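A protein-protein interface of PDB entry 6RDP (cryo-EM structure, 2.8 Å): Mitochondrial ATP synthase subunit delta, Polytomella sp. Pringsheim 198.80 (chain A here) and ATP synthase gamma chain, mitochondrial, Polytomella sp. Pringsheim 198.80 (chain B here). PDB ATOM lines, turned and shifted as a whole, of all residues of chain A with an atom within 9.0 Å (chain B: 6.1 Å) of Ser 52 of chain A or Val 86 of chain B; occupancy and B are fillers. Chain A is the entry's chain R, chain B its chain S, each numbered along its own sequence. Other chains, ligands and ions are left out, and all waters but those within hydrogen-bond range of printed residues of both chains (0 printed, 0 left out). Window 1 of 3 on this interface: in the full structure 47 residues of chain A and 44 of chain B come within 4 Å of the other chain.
Printed residues of chain B within 4 Å of Ser 52 of chain A: Val 86 and Asp 91.
Of the printed residues of chain A, Val 86 of chain B touches Ser 52 (3.7 Å) and Thr 55 (3.8 Å).
Printed residues of chain B within 4 Å of Asp 143 of chain A: Pro 84 and Arg 87.
Printed residues of chain B within 4 Å of Pro 51 of chain A: Asp 91 (3.3 Å).
Printed residues of chain A within 4 Å of Leu 88 of chain B: Phe 135 (3.7 Å) and His 137 (3.8 Å).
The nearest printed residue of chain B that does not touch Pro 51 of chain A is Val 86 of chain B (4.1 Å).
The side-chain carboxylate of Asp 143 of chain A lies within hydrogen-bond range of a ring nitrogen (ND1) of His 137 of chain A.
The side-chain sulfur (SG) of Cys 145 of chain A sits at hydrogen-bond distance from the backbone carbonyl oxygen (O) of Asp 143 of chain A (3.3 Å).
O of Thr 55 of chain A sits at hydrogen-bond distance from NZ of Lys 58 of chain A (2.4 Å).
O of Phe 135 of chain A sits at hydrogen-bond distance from N of Asp 143 of chain A (2.9 Å).
The backbone carbonyl oxygen of Ser 52 of chain A sits at hydrogen-bond distance from the side-chain hydroxyl of Thr 55 of chain A.
The backbone NH (N) of Phe 50 of chain A is in hydrogen-bond range of the side-chain amide oxygen (OD1) of Asn 53 of chain A.
Of the 11 printed residues of chain B, 6 touch a printed residue of chain A.
Printed residues of chain A that touch a printed residue of chain B: Gly 29, Phe 50, Pro 51, Ser 52, Thr 55, Val 57, Lys 58, Ala 59, Phe 135, His 137, Asp 143 and Cys 145.
Along chain A the printed residues that touch a printed residue of chain B span positions 29 to 145.
Among the printed residues, 17 pairs touch across the chains.
Among the printed residues, Asp or Glu carboxylates within 4 Å of a Lys or Arg side-chain nitrogen of the other chain: Asp 143 of chain A with Arg 87 of chain B (2.4 Å).
The guanidinium group (NH1) of Arg 87 of chain B is in hydrogen-bond range of the backbone carbonyl oxygen (O) of Val 57 of chain A (3.4 Å).
OG of Ser 52 of chain A is in hydrogen-bond range of OD1 of Asp 91 of chain B, at 2.7 Å.
NE of Arg 87 of chain B lies within salt-bridge range of OD1 of Asp 143 of chain A, 3.0 Å away.
Among the printed residues, pairs that only touch across the chains: Gly 29 of chain A with Asp 91 of chain B (3.2 Å), Phe 50 of chain A with Asp 91 of chain B (3.4 Å), Pro 51 of chain A with Asp 91 of chain B (3.3 Å), Ser 52 of chain A with Val 86 of chain B (3.7 Å), Thr 55 of chain A with Asp 83 of chain B (3.4 Å), Thr 55 of chain A with Val 86 of chain B (3.8 Å), Lys 58 of chain A with Arg 87 of chain B (3.9 Å), Ala 59 of chain A with Arg 87 of chain B (3.3 Å), Phe 135 of chain A with Pro 84 of chain B (3.9 Å), Phe 135 of chain A with Leu 88 of chain B (3.7 Å), His 137 of chain A with Arg 87 of chain B (3.6 Å), His 137 of chain A with Leu 88 of chain B (3.8 Å), Asp 143 of chain A with Pro 84 of chain B (3.6 Å) and Cys 145 of chain A with Pro 84 of chain B (3.6 Å).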
ATOM      1  N   ALA A  28      19.156 -15.024  -7.248  1.00  0.00           N
ATOM      2  CA  ALA A  28      20.499 -15.490  -6.935  1.00  0.00           C
ATOM      3  C   ALA A  28      20.855 -15.149  -5.491  1.00  0.00           C
ATOM      4  O   ALA A  28      20.008 -14.780  -4.674  1.00  0.00           O
ATOM      5  CB  ALA A  28      21.512 -14.901  -7.907  1.00  0.00           C
ATOM      6  N   GLY A  29      22.132 -15.272  -5.168  1.00  0.00           N
ATOM      7  CA  GLY A  29      22.601 -15.086  -3.823  1.00  0.00           C
ATOM      8  C   GLY A  29      23.776 -15.994  -3.570  1.00  0.00           C
ATOM      9  O   GLY A  29      24.212 -16.732  -4.457  1.00  0.00           O
ATOM     10  N   PRO A  30      24.335 -15.940  -2.361  1.00  0.00           N
ATOM     11  CA  PRO A  30      25.352 -16.940  -2.008  1.00  0.00           C
ATOM     12  C   PRO A  30      24.775 -18.335  -1.899  1.00  0.00           C
ATOM     13  O   PRO A  30      25.416 -19.303  -2.331  1.00  0.00           O
ATOM     14  CB  PRO A  30      25.894 -16.431  -0.663  1.00  0.00           C
ATOM     15  CG  PRO A  30      24.840 -15.535  -0.127  1.00  0.00           C
ATOM     16  CD  PRO A  30      24.171 -14.916  -1.316  1.00  0.00           C
ATOM     17  N   LYS A  31      23.558 -18.458  -1.372  1.00  0.00           N
ATOM     18  CA  LYS A  31      22.950 -19.761  -1.151  1.00  0.00           C
ATOM     19  C   LYS A  31      22.511 -20.439  -2.441  1.00  0.00           C
ATOM     20  O   LYS A  31      22.654 -21.657  -2.551  1.00  0.00           O
ATOM     21  CB  LYS A  31      21.760 -19.622  -0.201  1.00  0.00           C
ATOM     22  CG  LYS A  31      22.176 -19.223   1.201  1.00  0.00           C
ATOM     23  CD  LYS A  31      20.995 -19.115   2.146  1.00  0.00           C
ATOM     24  CE  LYS A  31      21.450 -18.713   3.541  1.00  0.00           C
ATOM     25  NZ  LYS A  31      20.310 -18.615   4.489  1.00  0.00           N
ATOM     26  N   PRO A  48      33.322 -20.741  -3.820  1.00  0.00           N
ATOM     27  CA  PRO A  48      34.049 -19.474  -3.753  1.00  0.00           C
ATOM     28  C   PRO A  48      33.327 -18.506  -2.840  1.00  0.00           C
ATOM     29  O   PRO A  48      32.099 -18.483  -2.784  1.00  0.00           O
ATOM     30  CB  PRO A  48      34.051 -18.988  -5.206  1.00  0.00           C
ATOM     31  CG  PRO A  48      32.929 -19.679  -5.839  1.00  0.00           C
ATOM     32  CD  PRO A  48      32.846 -21.016  -5.185  1.00  0.00           C
ATOM     33  N   GLU A  49      34.098 -17.733  -2.092  1.00  0.00           N
ATOM     34  CA  GLU A  49      33.493 -16.819  -1.148  1.00  0.00           C
ATOM     35  C   GLU A  49      32.865 -15.640  -1.873  1.00  0.00           C
ATOM     36  O   GLU A  49      33.084 -15.411  -3.065  1.00  0.00           O
ATOM     37  CB  GLU A  49      34.515 -16.337  -0.135  1.00  0.00           C
ATOM     38  CG  GLU A  49      34.786 -17.347   0.940  1.00  0.00           C
ATOM     39  CD  GLU A  49      33.540 -17.725   1.716  1.00  0.00           C
ATOM     40  OE1 GLU A  49      33.120 -16.938   2.586  1.00  0.00           O
ATOM     41  OE2 GLU A  49      32.971 -18.807   1.450  1.00  0.00           O
ATOM     42  N   PHE A  50      32.048 -14.907  -1.142  1.00  0.00           N
ATOM     43  CA  PHE A  50      31.283 -13.789  -1.665  1.00  0.00           C
ATOM     44  C   PHE A  50      31.499 -12.590  -0.763  1.00  0.00           C
ATOM     45  O   PHE A  50      31.848 -12.746   0.411  1.00  0.00           O
ATOM     46  CB  PHE A  50      29.798 -14.156  -1.736  1.00  0.00           C
ATOM     47  CG  PHE A  50      29.527 -15.373  -2.547  1.00  0.00           C
ATOM     48  CD1 PHE A  50      29.260 -16.577  -1.934  1.00  0.00           C
ATOM     49  CD2 PHE A  50      29.545 -15.315  -3.930  1.00  0.00           C
ATOM     50  CE1 PHE A  50      29.006 -17.699  -2.681  1.00  0.00           C
ATOM     51  CE2 PHE A  50      29.294 -16.432  -4.682  1.00  0.00           C
ATOM     52  CZ  PHE A  50      29.028 -17.628  -4.055  1.00  0.00           C
ATOM     53  N   PRO A  51      31.306 -11.373  -1.281  1.00  0.00           N
ATOM     54  CA  PRO A  51      31.417 -10.179  -0.426  1.00  0.00           C
ATOM     55  C   PRO A  51      30.372 -10.094   0.678  1.00  0.00           C
ATOM     56  O   PRO A  51      30.543  -9.288   1.601  1.00  0.00           O
ATOM     57  CB  PRO A  51      31.257  -9.023  -1.419  1.00  0.00           C
ATOM     58  CG  PRO A  51      30.705  -9.639  -2.659  1.00  0.00           C
ATOM     59  CD  PRO A  51      31.256 -11.009  -2.704  1.00  0.00           C
ATOM     60  N   SER A  52      29.311 -10.899   0.620  1.00  0.00           N
ATOM     61  CA  SER A  52      28.327 -10.914   1.692  1.00  0.00           C
ATOM     62  C   SER A  52      28.879 -11.547   2.957  1.00  0.00           C
ATOM     63  O   SER A  52      28.406 -11.245   4.056  1.00  0.00           O
ATOM     64  CB  SER A  52      27.090 -11.672   1.233  1.00  0.00           C
ATOM     65  OG  SER A  52      26.617 -11.121   0.031  1.00  0.00           O
ATOM     66  N   ASN A  53      29.876 -12.413   2.827  1.00  0.00           N
ATOM     67  CA  ASN A  53      30.344 -13.220   3.944  1.00  0.00           C
ATOM     68  C   ASN A  53      31.231 -12.455   4.915  1.00  0.00           C
ATOM     69  O   ASN A  53      31.623 -13.019   5.940  1.00  0.00           O
ATOM     70  CB  ASN A  53      31.089 -14.446   3.414  1.00  0.00           C
ATOM     71  CG  ASN A  53      30.354 -15.121   2.272  1.00  0.00           C
ATOM     72  OD1 ASN A  53      30.942 -15.426   1.240  1.00  0.00           O
ATOM     73  ND2 ASN A  53      29.060 -15.355   2.455  1.00  0.00           N
ATOM     74  N   TYR A  54      31.557 -11.197   4.635  1.00  0.00           N
ATOM     75  CA  TYR A  54      32.409 -10.419   5.522  1.00  0.00           C
ATOM     76  C   TYR A  54      31.695  -9.189   6.057  1.00  0.00           C
ATOM     77  O   TYR A  54      32.329  -8.312   6.649  1.00  0.00           O
ATOM     78  CB  TYR A  54      33.701 -10.037   4.802  1.00  0.00           C
ATOM     79  CG  TYR A  54      34.311 -11.211   4.075  1.00  0.00           C
ATOM     80  CD1 TYR A  54      34.832 -12.290   4.783  1.00  0.00           C
ATOM     81  CD2 TYR A  54      34.341 -11.257   2.686  1.00  0.00           C
ATOM     82  CE1 TYR A  54      35.376 -13.374   4.131  1.00  0.00           C
ATOM     83  CE2 TYR A  54      34.887 -12.339   2.026  1.00  0.00           C
ATOM     84  CZ  TYR A  54      35.402 -13.392   2.756  1.00  0.00           C
ATOM     85  OH  TYR A  54      35.951 -14.469   2.113  1.00  0.00           O
ATOM     86  N   THR A  55      30.380  -9.117   5.875  1.00  0.00           N
ATOM     87  CA  THR A  55      29.559  -8.029   6.379  1.00  0.00           C
ATOM     88  C   THR A  55      28.525  -8.596   7.336  1.00  0.00           C
ATOM     89  O   THR A  55      27.721  -9.450   6.949  1.00  0.00           O
ATOM     90  CB  THR A  55      28.856  -7.293   5.240  1.00  0.00           C
ATOM     91  OG1 THR A  55      27.984  -8.203   4.560  1.00  0.00           O
ATOM     92  CG2 THR A  55      29.868  -6.748   4.253  1.00  0.00           C
ATOM     93  N   ALA A  56      28.553  -8.127   8.581  1.00  0.00           N
ATOM     94  CA  ALA A  56      27.513  -8.452   9.544  1.00  0.00           C
ATOM     95  C   ALA A  56      26.364  -7.463   9.510  1.00  0.00           C
ATOM     96  O   ALA A  56      25.325  -7.718  10.127  1.00  0.00           O
ATOM     97  CB  ALA A  56      28.085  -8.500  10.965  1.00  0.00           C
ATOM     98  N   VAL A  57      26.534  -6.348   8.808  1.00  0.00           N
ATOM     99  CA  VAL A  57      25.551  -5.276   8.753  1.00  0.00           C
ATOM    100  C   VAL A  57      24.922  -5.279   7.371  1.00  0.00           C
ATOM    101  O   VAL A  57      25.626  -5.356   6.359  1.00  0.00           O
ATOM    102  CB  VAL A  57      26.195  -3.917   9.058  1.00  0.00           C
ATOM    103  CG1 VAL A  57      25.125  -2.900   9.391  1.00  0.00           C
ATOM    104  CG2 VAL A  57      27.198  -4.053  10.187  1.00  0.00           C
ATOM    105  N   LYS A  58      23.601  -5.214   7.329  1.00  0.00           N
ATOM    106  CA  LYS A  58      22.848  -5.106   6.091  1.00  0.00           C
ATOM    107  C   LYS A  58      21.977  -3.853   6.140  1.00  0.00           C
ATOM    108  O   LYS A  58      22.079  -3.030   7.055  1.00  0.00           O
ATOM    109  CB  LYS A  58      22.009  -6.364   5.860  1.00  0.00           C
ATOM    110  CG  LYS A  58      22.699  -7.435   5.026  1.00  0.00           C
ATOM    111  CD  LYS A  58      23.727  -8.217   5.836  1.00  0.00           C
ATOM    112  CE  LYS A  58      24.578  -9.111   4.953  1.00  0.00           C
ATOM    113  NZ  LYS A  58      25.649  -9.800   5.726  1.00  0.00           N
ATOM    114  N   ALA A  59      21.116  -3.703   5.138  1.00  0.00           N
ATOM    115  CA  ALA A  59      20.187  -2.581   5.127  1.00  0.00           C
ATOM    116  C   ALA A  59      18.829  -2.961   5.697  1.00  0.00           C
ATOM    117  O   ALA A  59      18.261  -2.223   6.507  1.00  0.00           O
ATOM    118  CB  ALA A  59      20.015  -2.043   3.708  1.00  0.00           C
ATOM    119  N   VAL A  60      18.293  -4.111   5.278  1.00  0.00           N
ATOM    120  CA  VAL A  60      16.962  -4.518   5.715  1.00  0.00           C
ATOM    121  C   VAL A  60      16.961  -5.137   7.101  1.00  0.00           C
ATOM    122  O   VAL A  60      15.881  -5.358   7.666  1.00  0.00           O
ATOM    123  CB  VAL A  60      16.346  -5.504   4.707  1.00  0.00           C
ATOM    124  CG1 VAL A  60      16.346  -4.898   3.311  1.00  0.00           C
ATOM    125  CG2 VAL A  60      17.101  -6.823   4.724  1.00  0.00           C
ATOM    126  N   PHE A 135      24.960   6.979   1.376  1.00  0.00           N
ATOM    127  CA  PHE A 135      23.694   6.276   1.488  1.00  0.00           C
ATOM    128  C   PHE A 135      23.224   6.288   2.928  1.00  0.00           C
ATOM    129  O   PHE A 135      24.033   6.239   3.853  1.00  0.00           O
ATOM    130  CB  PHE A 135      23.825   4.832   1.023  1.00  0.00           C
ATOM    131  CG  PHE A 135      24.784   4.652  -0.098  1.00  0.00           C
ATOM    132  CD1 PHE A 135      24.507   5.159  -1.347  1.00  0.00           C
ATOM    133  CD2 PHE A 135      25.966   3.966   0.096  1.00  0.00           C
ATOM    134  CE1 PHE A 135      25.389   4.993  -2.375  1.00  0.00           C
ATOM    135  CE2 PHE A 135      26.850   3.796  -0.931  1.00  0.00           C
ATOM    136  CZ  PHE A 135      26.561   4.310  -2.170  1.00  0.00           C
ATOM    137  N   HIS A 137      20.452   3.905   4.965  1.00  0.00           N
ATOM    138  CA  HIS A 137      19.731   2.660   4.759  1.00  0.00           C
ATOM    139  C   HIS A 137      18.508   2.608   5.665  1.00  0.00           C
ATOM    140  O   HIS A 137      18.356   3.453   6.550  1.00  0.00           O
ATOM    141  CB  HIS A 137      20.692   1.499   4.995  1.00  0.00           C
ATOM    142  CG  HIS A 137      21.668   1.302   3.884  1.00  0.00           C
ATOM    143  ND1 HIS A 137      23.026   1.463   4.046  1.00  0.00           N
ATOM    144  CD2 HIS A 137      21.477   0.986   2.583  1.00  0.00           C
ATOM    145  CE1 HIS A 137      23.630   1.237   2.893  1.00  0.00           C
ATOM    146  NE2 HIS A 137      22.713   0.946   1.991  1.00  0.00           N
ATOM    147  N   ASP A 143      26.487   5.363   5.161  1.00  0.00           N
ATOM    148  CA  ASP A 143      27.748   4.981   4.542  1.00  0.00           C
ATOM    149  C   ASP A 143      28.196   6.099   3.622  1.00  0.00           C
ATOM    150  O   ASP A 143      27.789   6.153   2.463  1.00  0.00           O
ATOM    151  CB  ASP A 143      27.576   3.723   3.799  1.00  0.00           C
ATOM    152  CG  ASP A 143      26.949   2.659   4.633  1.00  0.00           C
ATOM    153  OD1 ASP A 143      27.687   1.923   5.310  1.00  0.00           O
ATOM    154  OD2 ASP A 143      25.711   2.583   4.643  1.00  0.00           O
ATOM    155  N   CYS A 145      30.698   7.615   1.184  1.00  0.00           N
ATOM    156  CA  CYS A 145      31.571   6.879   0.270  1.00  0.00           C
ATOM    157  C   CYS A 145      32.203   7.853  -0.713  1.00  0.00           C
ATOM    158  O   CYS A 145      31.682   8.060  -1.806  1.00  0.00           O
ATOM    159  CB  CYS A 145      30.778   5.826  -0.464  1.00  0.00           C
ATOM    160  SG  CYS A 145      29.972   4.637   0.579  1.00  0.00           S
ATOM    161  N   VAL B  82      33.746  -1.845   0.221  1.00  0.00           N
ATOM    162  CA  VAL B  82      33.002  -2.861  -0.513  1.00  0.00           C
ATOM    163  C   VAL B  82      31.670  -3.144   0.170  1.00  0.00           C
ATOM    164  O   VAL B  82      30.701  -3.559  -0.472  1.00  0.00           O
ATOM    165  CB  VAL B  82      33.854  -4.137  -0.650  1.00  0.00           C
ATOM    166  CG1 VAL B  82      33.307  -5.045  -1.740  1.00  0.00           C
ATOM    167  CG2 VAL B  82      35.289  -3.775  -0.932  1.00  0.00           C
ATOM    168  N   ASP B  83      31.599  -2.912   1.477  1.00  0.00           N
ATOM    169  CA  ASP B  83      30.416  -3.216   2.280  1.00  0.00           C
ATOM    170  C   ASP B  83      29.172  -2.362   1.994  1.00  0.00           C
ATOM    171  O   ASP B  83      28.072  -2.934   2.007  1.00  0.00           O
ATOM    172  CB  ASP B  83      30.758  -3.130   3.770  1.00  0.00           C
ATOM    173  CG  ASP B  83      32.025  -3.872   4.121  1.00  0.00           C
ATOM    174  OD1 ASP B  83      32.440  -4.744   3.334  1.00  0.00           O
ATOM    175  OD2 ASP B  83      32.602  -3.593   5.191  1.00  0.00           O
ATOM    176  N   PRO B  84      29.245  -1.032   1.774  1.00  0.00           N
ATOM    177  CA  PRO B  84      28.010  -0.307   1.437  1.00  0.00           C
ATOM    178  C   PRO B  84      27.389  -0.722   0.129  1.00  0.00           C
ATOM    179  O   PRO B  84      26.161  -0.700  -0.001  1.00  0.00           O
ATOM    180  CB  PRO B  84      28.465   1.155   1.380  1.00  0.00           C
ATOM    181  CG  PRO B  84      29.890   1.102   1.255  1.00  0.00           C
ATOM    182  CD  PRO B  84      30.297  -0.042   2.059  1.00  0.00           C
ATOM    183  N   PHE B  85      28.193  -1.127  -0.838  1.00  0.00           N
ATOM    184  CA  PHE B  85      27.624  -1.549  -2.101  1.00  0.00           C
ATOM    185  C   PHE B  85      27.003  -2.926  -2.006  1.00  0.00           C
ATOM    186  O   PHE B  85      26.074  -3.228  -2.760  1.00  0.00           O
ATOM    187  CB  PHE B  85      28.692  -1.515  -3.174  1.00  0.00           C
ATOM    188  CG  PHE B  85      29.150  -0.145  -3.499  1.00  0.00           C
ATOM    189  CD1 PHE B  85      28.439   0.632  -4.382  1.00  0.00           C
ATOM    190  CD2 PHE B  85      30.278   0.379  -2.905  1.00  0.00           C
ATOM    191  CE1 PHE B  85      28.854   1.896  -4.677  1.00  0.00           C
ATOM    192  CE2 PHE B  85      30.693   1.648  -3.196  1.00  0.00           C
ATOM    193  CZ  PHE B  85      29.981   2.402  -4.081  1.00  0.00           C
ATOM    194  N   VAL B  86      27.473  -3.772  -1.097  1.00  0.00           N
ATOM    195  CA  VAL B  86      26.827  -5.068  -0.963  1.00  0.00           C
ATOM    196  C   VAL B  86      25.598  -4.977  -0.065  1.00  0.00           C
ATOM    197  O   VAL B  86      24.629  -5.717  -0.284  1.00  0.00           O
ATOM    198  CB  VAL B  86      27.823  -6.153  -0.500  1.00  0.00           C
ATOM    199  CG1 VAL B  86      28.203  -6.019   0.961  1.00  0.00           C
ATOM    200  CG2 VAL B  86      27.272  -7.537  -0.794  1.00  0.00           C
ATOM    201  N   ARG B  87      25.565  -4.044   0.882  1.00  0.00           N
ATOM    202  CA  ARG B  87      24.336  -3.856   1.631  1.00  0.00           C
ATOM    203  C   ARG B  87      23.386  -2.893   0.942  1.00  0.00           C
ATOM    204  O   ARG B  87      22.304  -2.635   1.466  1.00  0.00           O
ATOM    205  CB  ARG B  87      24.627  -3.385   3.052  1.00  0.00           C
ATOM    206  CG  ARG B  87      25.167  -2.001   3.176  1.00  0.00           C
ATOM    207  CD  ARG B  87      25.108  -1.576   4.617  1.00  0.00           C
ATOM    208  NE  ARG B  87      26.221  -0.721   4.996  1.00  0.00           N
ATOM    209  CZ  ARG B  87      27.250  -1.132   5.718  1.00  0.00           C
ATOM    210  NH1 ARG B  87      27.307  -2.387   6.127  1.00  0.00           N
ATOM    211  NH2 ARG B  87      28.223  -0.291   6.026  1.00  0.00           N
ATOM    212  N   LEU B  88      23.765  -2.353  -0.211  1.00  0.00           N
ATOM    213  CA  LEU B  88      22.838  -1.578  -1.021  1.00  0.00           C
ATOM    214  C   LEU B  88      22.334  -2.378  -2.215  1.00  0.00           C
ATOM    215  O   LEU B  88      21.133  -2.391  -2.495  1.00  0.00           O
ATOM    216  CB  LEU B  88      23.503  -0.284  -1.489  1.00  0.00           C
ATOM    217  CG  LEU B  88      22.661   0.640  -2.363  1.00  0.00           C
ATOM    218  CD1 LEU B  88      21.390   1.005  -1.643  1.00  0.00           C
ATOM    219  CD2 LEU B  88      23.436   1.886  -2.713  1.00  0.00           C
ATOM    220  N   PHE B  89      23.234  -3.055  -2.924  1.00  0.00           N
ATOM    221  CA  PHE B  89      22.893  -3.725  -4.169  1.00  0.00           C
ATOM    222  C   PHE B  89      22.755  -5.229  -4.033  1.00  0.00           C
ATOM    223  O   PHE B  89      22.140  -5.858  -4.900  1.00  0.00           O
ATOM    224  CB  PHE B  89      23.951  -3.435  -5.232  1.00  0.00           C
ATOM    225  CG  PHE B  89      23.908  -2.048  -5.770  1.00  0.00           C
ATOM    226  CD1 PHE B  89      22.784  -1.262  -5.615  1.00  0.00           C
ATOM    227  CD2 PHE B  89      24.994  -1.534  -6.447  1.00  0.00           C
ATOM    228  CE1 PHE B  89      22.751   0.010  -6.116  1.00  0.00           C
ATOM    229  CE2 PHE B  89      24.965  -0.260  -6.955  1.00  0.00           C
ATOM    230  CZ  PHE B  89      23.843   0.508  -6.792  1.00  0.00           C
ATOM    231  N   GLY B  90      23.311  -5.823  -2.991  1.00  0.00           N
ATOM    232  CA  GLY B  90      23.212  -7.254  -2.827  1.00  0.00           C
ATOM    233  C   GLY B  90      24.192  -8.018  -3.701  1.00  0.00           C
ATOM    234  O   GLY B  90      25.014  -7.455  -4.429  1.00  0.00           O
ATOM    235  N   ASP B  91      24.051  -9.340  -3.653  1.00  0.00           N
ATOM    236  CA  ASP B  91      25.054 -10.270  -4.169  1.00  0.00           C
ATOM    237  C   ASP B  91      24.351 -11.210  -5.137  1.00  0.00           C
ATOM    238  O   ASP B  91      23.701 -12.165  -4.711  1.00  0.00           O
ATOM    239  CB  ASP B  91      25.678 -11.049  -3.024  1.00  0.00           C
ATOM    240  CG  ASP B  91      27.115 -11.401  -3.267  1.00  0.00           C
ATOM    241  OD1 ASP B  91      27.897 -11.358  -2.297  1.00  0.00           O
ATOM    242  OD2 ASP B  91      27.461 -11.718  -4.416  1.00  0.00           O
ATOM    243  N   HIS B 250      30.989   1.206  -8.039  1.00  0.00           N
ATOM    244  CA  HIS B 250      31.045  -0.119  -7.432  1.00  0.00           C
ATOM    245  C   HIS B 250      32.043  -1.020  -8.140  1.00  0.00           C
ATOM    246  O   HIS B 250      32.736  -1.814  -7.494  1.00  0.00           O
ATOM    247  CB  HIS B 250      29.655  -0.735  -7.446  1.00  0.00           C
ATOM    248  CG  HIS B 250      29.593  -2.120  -6.893  1.00  0.00           C
ATOM    249  ND1 HIS B 250      30.370  -2.530  -5.836  1.00  0.00           N
ATOM    250  CD2 HIS B 250      28.775  -3.155  -7.182  1.00  0.00           C
ATOM    251  CE1 HIS B 250      30.073  -3.781  -5.533  1.00  0.00           C
ATOM    252  NE2 HIS B 250      29.102  -4.181  -6.332  1.00  0.00           N
